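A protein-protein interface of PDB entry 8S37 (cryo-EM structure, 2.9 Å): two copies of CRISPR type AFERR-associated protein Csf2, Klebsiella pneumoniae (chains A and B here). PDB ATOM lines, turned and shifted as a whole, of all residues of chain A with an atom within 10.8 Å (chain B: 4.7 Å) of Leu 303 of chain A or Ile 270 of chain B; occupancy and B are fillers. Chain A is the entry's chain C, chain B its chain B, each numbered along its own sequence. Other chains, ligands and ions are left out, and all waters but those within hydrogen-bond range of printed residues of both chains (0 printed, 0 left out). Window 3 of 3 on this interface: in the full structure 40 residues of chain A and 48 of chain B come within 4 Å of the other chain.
O of Leu 303 of chain A is in hydrogen-bond range of N of Val 318 of chain B (2.7 Å).
O of Glu 302 of chain A is in hydrogen-bond range of NE1 of Trp 298 of chain A (2.6 Å).
O of Ala 273 of chain B touches CZ3 of Trp 298 of chain A, at 3.4 Å.
CD2 of Trp 298 of chain A touches CA of Ala 274 of chain B, at 3.8 Å.
CA of Gly 317 of chain B touches CH2 of Trp 298 of chain A, 3.5 Å away.
Trp 298 of chain A touches Val 318 of chain B (CZ2 to CG2, 3.8 Å).
CB of Pro 300 of chain A touches CZ of Arg 271 of chain B (3.4 Å).
Pro 300 of chain A touches Ala 274 of chain B.
Ile 270 of chain B touches Gly 301 of chain A (CG2 to O, 3.8 Å).
Leu 303 of chain A touches Ile 270 of chain B (CD2 to CG1, 3.5 Å).
Gly 317 of chain B touches Leu 303 of chain A.
Pro 305 of chain A touches Gly 317 of chain B (CD to N, 3.8 Å).
Thr 297 of chain A touches none of the printed residues of chain B.
Printed residues of chain B within 4 Å of Trp 298 of chain A: Ala 273, Ala 274, Gly 317 and Val 318.
Printed residues of chain B within 4 Å of Gly 301 of chain A: Ile 270.
Leu 303 of chain A touches just these residues of chain B: Ile 270, Gly 317 and Val 318.
No residue of chain A comes within 4 Å of Ser 267 of chain B.
No residue of chain A comes within 4 Å of Ala 268 of chain B.
No residue of chain A comes within 4 Å of Leu 269 of chain B.
Ile 270 of chain B touches two residues of chain A.
Of the printed residues of chain A, Arg 271 of chain B touches Pro 300.
Of chain A, only Trp 298 comes within 4 Å of Ala 273 of chain B.
Printed residues of chain A within 4 Å of Ala 274 of chain B: Trp 298 (3.8 Å) and Pro 300 (3.8 Å).
The nearest residue of chain B that does not touch Leu 303 of chain A is Ile 320 of chain B (4.5 Å).
The nearest residue of chain A that does not touch Ile 270 of chain B is Glu 302 of chain A (4.5 Å).
The nearest printed residue of chain B that does not touch Trp 298 of chain A is Ile 270 of chain B (5.3 Å).
Printed residues of chain A that touch a printed residue of chain B: Trp 298, Pro 300, Gly 301, Leu 303 and Pro 305.
Hydrophobic or aromatic side chains of chain B within 4 Å of the printed part of chain A: Ile 270, Ala 274 and Val 318.
Among the printed residues, no Asp or Glu carboxylate lies within 4 Å of a Lys or Arg side-chain nitrogen of the other chain.
No position is printed for both chains.
Of the 11 pairs that touch across the chains among the printed residues, none has its exchanged pair printed and touching as well.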
ATOM      1  N   THR A   3     -15.949   0.113 -23.976  1.00  0.00           N
ATOM      2  CA  THR A   3     -16.645   1.390 -23.917  1.00  0.00           C
ATOM      3  C   THR A   3     -15.687   2.471 -23.440  1.00  0.00           C
ATOM      4  O   THR A   3     -15.022   2.301 -22.415  1.00  0.00           O
ATOM      5  CB  THR A   3     -17.849   1.304 -22.981  1.00  0.00           C
ATOM      6  OG1 THR A   3     -18.721   0.254 -23.415  1.00  0.00           O
ATOM      7  CG2 THR A   3     -18.612   2.618 -22.969  1.00  0.00           C
ATOM      8  N   THR A 297     -12.493   3.940 -19.214  1.00  0.00           N
ATOM      9  CA  THR A 297     -13.063   2.717 -19.750  1.00  0.00           C
ATOM     10  C   THR A 297     -13.651   1.912 -18.604  1.00  0.00           C
ATOM     11  O   THR A 297     -13.298   2.107 -17.439  1.00  0.00           O
ATOM     12  CB  THR A 297     -12.018   1.880 -20.496  1.00  0.00           C
ATOM     13  OG1 THR A 297     -12.671   0.823 -21.206  1.00  0.00           O
ATOM     14  CG2 THR A 297     -11.011   1.280 -19.523  1.00  0.00           C
ATOM     15  N   TRP A 298     -14.568   1.010 -18.941  1.00  0.00           N
ATOM     16  CA  TRP A 298     -15.282   0.253 -17.917  1.00  0.00           C
ATOM     17  C   TRP A 298     -15.571  -1.132 -18.485  1.00  0.00           C
ATOM     18  O   TRP A 298     -16.529  -1.309 -19.242  1.00  0.00           O
ATOM     19  CB  TRP A 298     -16.556   0.975 -17.507  1.00  0.00           C
ATOM     20  CG  TRP A 298     -17.041   0.627 -16.139  1.00  0.00           C
ATOM     21  CD1 TRP A 298     -16.850  -0.545 -15.473  1.00  0.00           C
ATOM     22  CD2 TRP A 298     -17.791   1.470 -15.262  1.00  0.00           C
ATOM     23  NE1 TRP A 298     -17.439  -0.488 -14.236  1.00  0.00           N
ATOM     24  CE2 TRP A 298     -18.025   0.741 -14.082  1.00  0.00           C
ATOM     25  CE3 TRP A 298     -18.291   2.770 -15.360  1.00  0.00           C
ATOM     26  CZ2 TRP A 298     -18.735   1.266 -13.011  1.00  0.00           C
ATOM     27  CZ3 TRP A 298     -18.998   3.291 -14.295  1.00  0.00           C
ATOM     28  CH2 TRP A 298     -19.214   2.540 -13.136  1.00  0.00           C
ATOM     29  N   LYS A 299     -14.743  -2.095 -18.119  1.00  0.00           N
ATOM     30  CA  LYS A 299     -14.987  -3.471 -18.515  1.00  0.00           C
ATOM     31  C   LYS A 299     -16.276  -3.937 -17.847  1.00  0.00           C
ATOM     32  O   LYS A 299     -16.368  -3.870 -16.615  1.00  0.00           O
ATOM     33  CB  LYS A 299     -13.825  -4.366 -18.110  1.00  0.00           C
ATOM     34  CG  LYS A 299     -13.900  -5.761 -18.713  1.00  0.00           C
ATOM     35  CD  LYS A 299     -12.687  -6.611 -18.355  1.00  0.00           C
ATOM     36  CE  LYS A 299     -12.660  -7.005 -16.883  1.00  0.00           C
ATOM     37  NZ  LYS A 299     -13.868  -7.773 -16.470  1.00  0.00           N
ATOM     38  N   PRO A 300     -17.297  -4.366 -18.596  1.00  0.00           N
ATOM     39  CA  PRO A 300     -18.541  -4.797 -17.948  1.00  0.00           C
ATOM     40  C   PRO A 300     -18.291  -5.879 -16.909  1.00  0.00           C
ATOM     41  O   PRO A 300     -17.541  -6.829 -17.140  1.00  0.00           O
ATOM     42  CB  PRO A 300     -19.384  -5.320 -19.114  1.00  0.00           C
ATOM     43  CG  PRO A 300     -18.889  -4.590 -20.287  1.00  0.00           C
ATOM     44  CD  PRO A 300     -17.422  -4.398 -20.065  1.00  0.00           C
ATOM     45  N   GLY A 301     -18.928  -5.717 -15.752  1.00  0.00           N
ATOM     46  CA  GLY A 301     -18.711  -6.564 -14.605  1.00  0.00           C
ATOM     47  C   GLY A 301     -17.738  -6.005 -13.589  1.00  0.00           C
ATOM     48  O   GLY A 301     -17.717  -6.479 -12.448  1.00  0.00           O
ATOM     49  N   GLU A 302     -16.933  -5.016 -13.969  1.00  0.00           N
ATOM     50  CA  GLU A 302     -16.055  -4.352 -13.018  1.00  0.00           C
ATOM     51  C   GLU A 302     -16.819  -3.273 -12.262  1.00  0.00           C
ATOM     52  O   GLU A 302     -17.723  -2.629 -12.799  1.00  0.00           O
ATOM     53  CB  GLU A 302     -14.856  -3.731 -13.732  1.00  0.00           C
ATOM     54  CG  GLU A 302     -13.899  -4.742 -14.339  1.00  0.00           C
ATOM     55  CD  GLU A 302     -13.140  -5.536 -13.294  1.00  0.00           C
ATOM     56  OE1 GLU A 302     -13.280  -5.231 -12.092  1.00  0.00           O
ATOM     57  OE2 GLU A 302     -12.400  -6.467 -13.678  1.00  0.00           O
ATOM     58  N   LEU A 303     -16.443  -3.078 -11.002  1.00  0.00           N
ATOM     59  CA  LEU A 303     -17.105  -2.103 -10.149  1.00  0.00           C
ATOM     60  C   LEU A 303     -16.557  -0.690 -10.299  1.00  0.00           C
ATOM     61  O   LEU A 303     -17.196   0.251  -9.815  1.00  0.00           O
ATOM     62  CB  LEU A 303     -16.985  -2.529  -8.682  1.00  0.00           C
ATOM     63  CG  LEU A 303     -17.614  -3.876  -8.325  1.00  0.00           C
ATOM     64  CD1 LEU A 303     -17.192  -4.305  -6.931  1.00  0.00           C
ATOM     65  CD2 LEU A 303     -19.127  -3.807  -8.423  1.00  0.00           C
ATOM     66  N   VAL A 304     -15.405  -0.518 -10.945  1.00  0.00           N
ATOM     67  CA  VAL A 304     -14.791   0.805 -11.096  1.00  0.00           C
ATOM     68  C   VAL A 304     -14.313   0.981 -12.526  1.00  0.00           C
ATOM     69  O   VAL A 304     -13.929   0.010 -13.194  1.00  0.00           O
ATOM     70  CB  VAL A 304     -13.608   1.001 -10.129  1.00  0.00           C
ATOM     71  CG1 VAL A 304     -14.115   1.187  -8.711  1.00  0.00           C
ATOM     72  CG2 VAL A 304     -12.644  -0.180 -10.199  1.00  0.00           C
ATOM     73  N   PRO A 305     -14.321   2.215 -13.031  1.00  0.00           N
ATOM     74  CA  PRO A 305     -13.662   2.477 -14.312  1.00  0.00           C
ATOM     75  C   PRO A 305     -12.160   2.649 -14.146  1.00  0.00           C
ATOM     76  O   PRO A 305     -11.644   2.880 -13.051  1.00  0.00           O
ATOM     77  CB  PRO A 305     -14.308   3.779 -14.803  1.00  0.00           C
ATOM     78  CG  PRO A 305     -15.195   4.254 -13.706  1.00  0.00           C
ATOM     79  CD  PRO A 305     -14.903   3.455 -12.487  1.00  0.00           C
ATOM     80  N   VAL A 306     -11.462   2.532 -15.272  1.00  0.00           N
ATOM     81  CA  VAL A 306     -10.022   2.745 -15.359  1.00  0.00           C
ATOM     82  C   VAL A 306      -9.780   3.924 -16.287  1.00  0.00           C
ATOM     83  O   VAL A 306     -10.246   3.921 -17.431  1.00  0.00           O
ATOM     84  CB  VAL A 306      -9.293   1.489 -15.870  1.00  0.00           C
ATOM     85  CG1 VAL A 306      -7.784   1.676 -15.784  1.00  0.00           C
ATOM     86  CG2 VAL A 306      -9.734   0.263 -15.085  1.00  0.00           C
ATOM     87  N   ILE B 266     -28.463  -7.965  -8.959  1.00  0.00           N
ATOM     88  CA  ILE B 266     -27.450  -6.988  -8.583  1.00  0.00           C
ATOM     89  C   ILE B 266     -26.279  -7.038  -9.556  1.00  0.00           C
ATOM     90  O   ILE B 266     -25.686  -6.005  -9.884  1.00  0.00           O
ATOM     91  CB  ILE B 266     -26.997  -7.215  -7.131  1.00  0.00           C
ATOM     92  CG1 ILE B 266     -28.158  -6.952  -6.168  1.00  0.00           C
ATOM     93  CG2 ILE B 266     -25.825  -6.304  -6.801  1.00  0.00           C
ATOM     94  CD1 ILE B 266     -27.964  -7.545  -4.793  1.00  0.00           C
ATOM     95  N   SER B 267     -25.939  -8.228 -10.052  1.00  0.00           N
ATOM     96  CA  SER B 267     -24.885  -8.320 -11.057  1.00  0.00           C
ATOM     97  C   SER B 267     -25.319  -7.662 -12.359  1.00  0.00           C
ATOM     98  O   SER B 267     -24.502  -7.056 -13.062  1.00  0.00           O
ATOM     99  CB  SER B 267     -24.511  -9.781 -11.292  1.00  0.00           C
ATOM    100  OG  SER B 267     -24.005 -10.370 -10.109  1.00  0.00           O
ATOM    101  N   ALA B 268     -26.604  -7.768 -12.693  1.00  0.00           N
ATOM    102  CA  ALA B 268     -27.121  -7.089 -13.872  1.00  0.00           C
ATOM    103  C   ALA B 268     -27.034  -5.582 -13.706  1.00  0.00           C
ATOM    104  O   ALA B 268     -26.696  -4.863 -14.650  1.00  0.00           O
ATOM    105  CB  ALA B 268     -28.564  -7.516 -14.132  1.00  0.00           C
ATOM    106  N   LEU B 269     -27.348  -5.084 -12.511  1.00  0.00           N
ATOM    107  CA  LEU B 269     -27.181  -3.659 -12.244  1.00  0.00           C
ATOM    108  C   LEU B 269     -25.717  -3.254 -12.347  1.00  0.00           C
ATOM    109  O   LEU B 269     -25.395  -2.178 -12.864  1.00  0.00           O
ATOM    110  CB  LEU B 269     -27.734  -3.316 -10.861  1.00  0.00           C
ATOM    111  CG  LEU B 269     -29.255  -3.321 -10.720  1.00  0.00           C
ATOM    112  CD1 LEU B 269     -29.643  -3.306  -9.254  1.00  0.00           C
ATOM    113  CD2 LEU B 269     -29.867  -2.135 -11.442  1.00  0.00           C
ATOM    114  N   ILE B 270     -24.816  -4.111 -11.865  1.00  0.00           N
ATOM    115  CA  ILE B 270     -23.386  -3.818 -11.932  1.00  0.00           C
ATOM    116  C   ILE B 270     -22.938  -3.717 -13.383  1.00  0.00           C
ATOM    117  O   ILE B 270     -22.193  -2.804 -13.756  1.00  0.00           O
ATOM    118  CB  ILE B 270     -22.587  -4.877 -11.143  1.00  0.00           C
ATOM    119  CG1 ILE B 270     -22.323  -4.393  -9.712  1.00  0.00           C
ATOM    120  CG2 ILE B 270     -21.241  -5.211 -11.808  1.00  0.00           C
ATOM    121  CD1 ILE B 270     -23.559  -4.235  -8.845  1.00  0.00           C
ATOM    122  N   ARG B 271     -23.379  -4.650 -14.223  1.00  0.00           N
ATOM    123  CA  ARG B 271     -22.949  -4.627 -15.615  1.00  0.00           C
ATOM    124  C   ARG B 271     -23.610  -3.485 -16.371  1.00  0.00           C
ATOM    125  O   ARG B 271     -22.991  -2.891 -17.261  1.00  0.00           O
ATOM    126  CB  ARG B 271     -23.264  -5.955 -16.297  1.00  0.00           C
ATOM    127  CG  ARG B 271     -22.536  -6.134 -17.615  1.00  0.00           C
ATOM    128  CD  ARG B 271     -23.126  -7.246 -18.451  1.00  0.00           C
ATOM    129  NE  ARG B 271     -22.394  -7.408 -19.702  1.00  0.00           N
ATOM    130  CZ  ARG B 271     -21.263  -8.089 -19.831  1.00  0.00           C
ATOM    131  NH1 ARG B 271     -20.696  -8.699 -18.801  1.00  0.00           N
ATOM    132  NH2 ARG B 271     -20.682  -8.159 -21.025  1.00  0.00           N
ATOM    133  N   PHE B 272     -24.858  -3.166 -16.034  1.00  0.00           N
ATOM    134  CA  PHE B 272     -25.508  -1.999 -16.615  1.00  0.00           C
ATOM    135  C   PHE B 272     -24.756  -0.723 -16.272  1.00  0.00           C
ATOM    136  O   PHE B 272     -24.752   0.228 -17.061  1.00  0.00           O
ATOM    137  CB  PHE B 272     -26.954  -1.921 -16.122  1.00  0.00           C
ATOM    138  CG  PHE B 272     -27.534  -0.541 -16.154  1.00  0.00           C
ATOM    139  CD1 PHE B 272     -28.081  -0.033 -17.316  1.00  0.00           C
ATOM    140  CD2 PHE B 272     -27.541   0.247 -15.016  1.00  0.00           C
ATOM    141  CE1 PHE B 272     -28.619   1.234 -17.344  1.00  0.00           C
ATOM    142  CE2 PHE B 272     -28.070   1.515 -15.042  1.00  0.00           C
ATOM    143  CZ  PHE B 272     -28.605   2.012 -16.206  1.00  0.00           C
ATOM    144  N   ALA B 273     -24.108  -0.683 -15.107  1.00  0.00           N
ATOM    145  CA  ALA B 273     -23.347   0.496 -14.716  1.00  0.00           C
ATOM    146  C   ALA B 273     -22.189   0.773 -15.662  1.00  0.00           C
ATOM    147  O   ALA B 273     -21.730   1.915 -15.741  1.00  0.00           O
ATOM    148  CB  ALA B 273     -22.826   0.338 -13.294  1.00  0.00           C
ATOM    149  N   ALA B 274     -21.688  -0.249 -16.357  1.00  0.00           N
ATOM    150  CA  ALA B 274     -20.624  -0.023 -17.329  1.00  0.00           C
ATOM    151  C   ALA B 274     -21.102   0.888 -18.450  1.00  0.00           C
ATOM    152  O   ALA B 274     -20.375   1.792 -18.878  1.00  0.00           O
ATOM    153  CB  ALA B 274     -20.135  -1.356 -17.891  1.00  0.00           C
ATOM    154  N   GLY B 317     -17.901   4.647 -10.479  1.00  0.00           N
ATOM    155  CA  GLY B 317     -17.933   3.278 -10.007  1.00  0.00           C
ATOM    156  C   GLY B 317     -19.301   2.895  -9.483  1.00  0.00           C
ATOM    157  O   GLY B 317     -20.245   3.687  -9.473  1.00  0.00           O
ATOM    158  N   VAL B 318     -19.384   1.641  -9.049  1.00  0.00           N
ATOM    159  CA  VAL B 318     -20.568   1.094  -8.403  1.00  0.00           C
ATOM    160  C   VAL B 318     -20.207   0.862  -6.945  1.00  0.00           C
ATOM    161  O   VAL B 318     -19.353   0.027  -6.628  1.00  0.00           O
ATOM    162  CB  VAL B 318     -21.037  -0.207  -9.064  1.00  0.00           C
ATOM    163  CG1 VAL B 318     -22.284  -0.732  -8.370  1.00  0.00           C
ATOM    164  CG2 VAL B 318     -21.295   0.017 -10.530  1.00  0.00           C
ATOM    165  N   ILE B 320     -21.483  -0.453  -3.440  1.00  0.00           N
ATOM    166  CA  ILE B 320     -22.466  -1.314  -2.799  1.00  0.00           C
ATOM    167  C   ILE B 320     -22.167  -1.305  -1.312  1.00  0.00           C
ATOM    168  O   ILE B 320     -21.087  -1.735  -0.888  1.00  0.00           O
ATOM    169  CB  ILE B 320     -22.422  -2.744  -3.358  1.00  0.00           C
ATOM    170  CG1 ILE B 320     -22.850  -2.759  -4.826  1.00  0.00           C
ATOM    171  CG2 ILE B 320     -23.308  -3.657  -2.521  1.00  0.00           C
ATOM    172  CD1 ILE B 320     -22.530  -4.055  -5.537  1.00  0.00           C
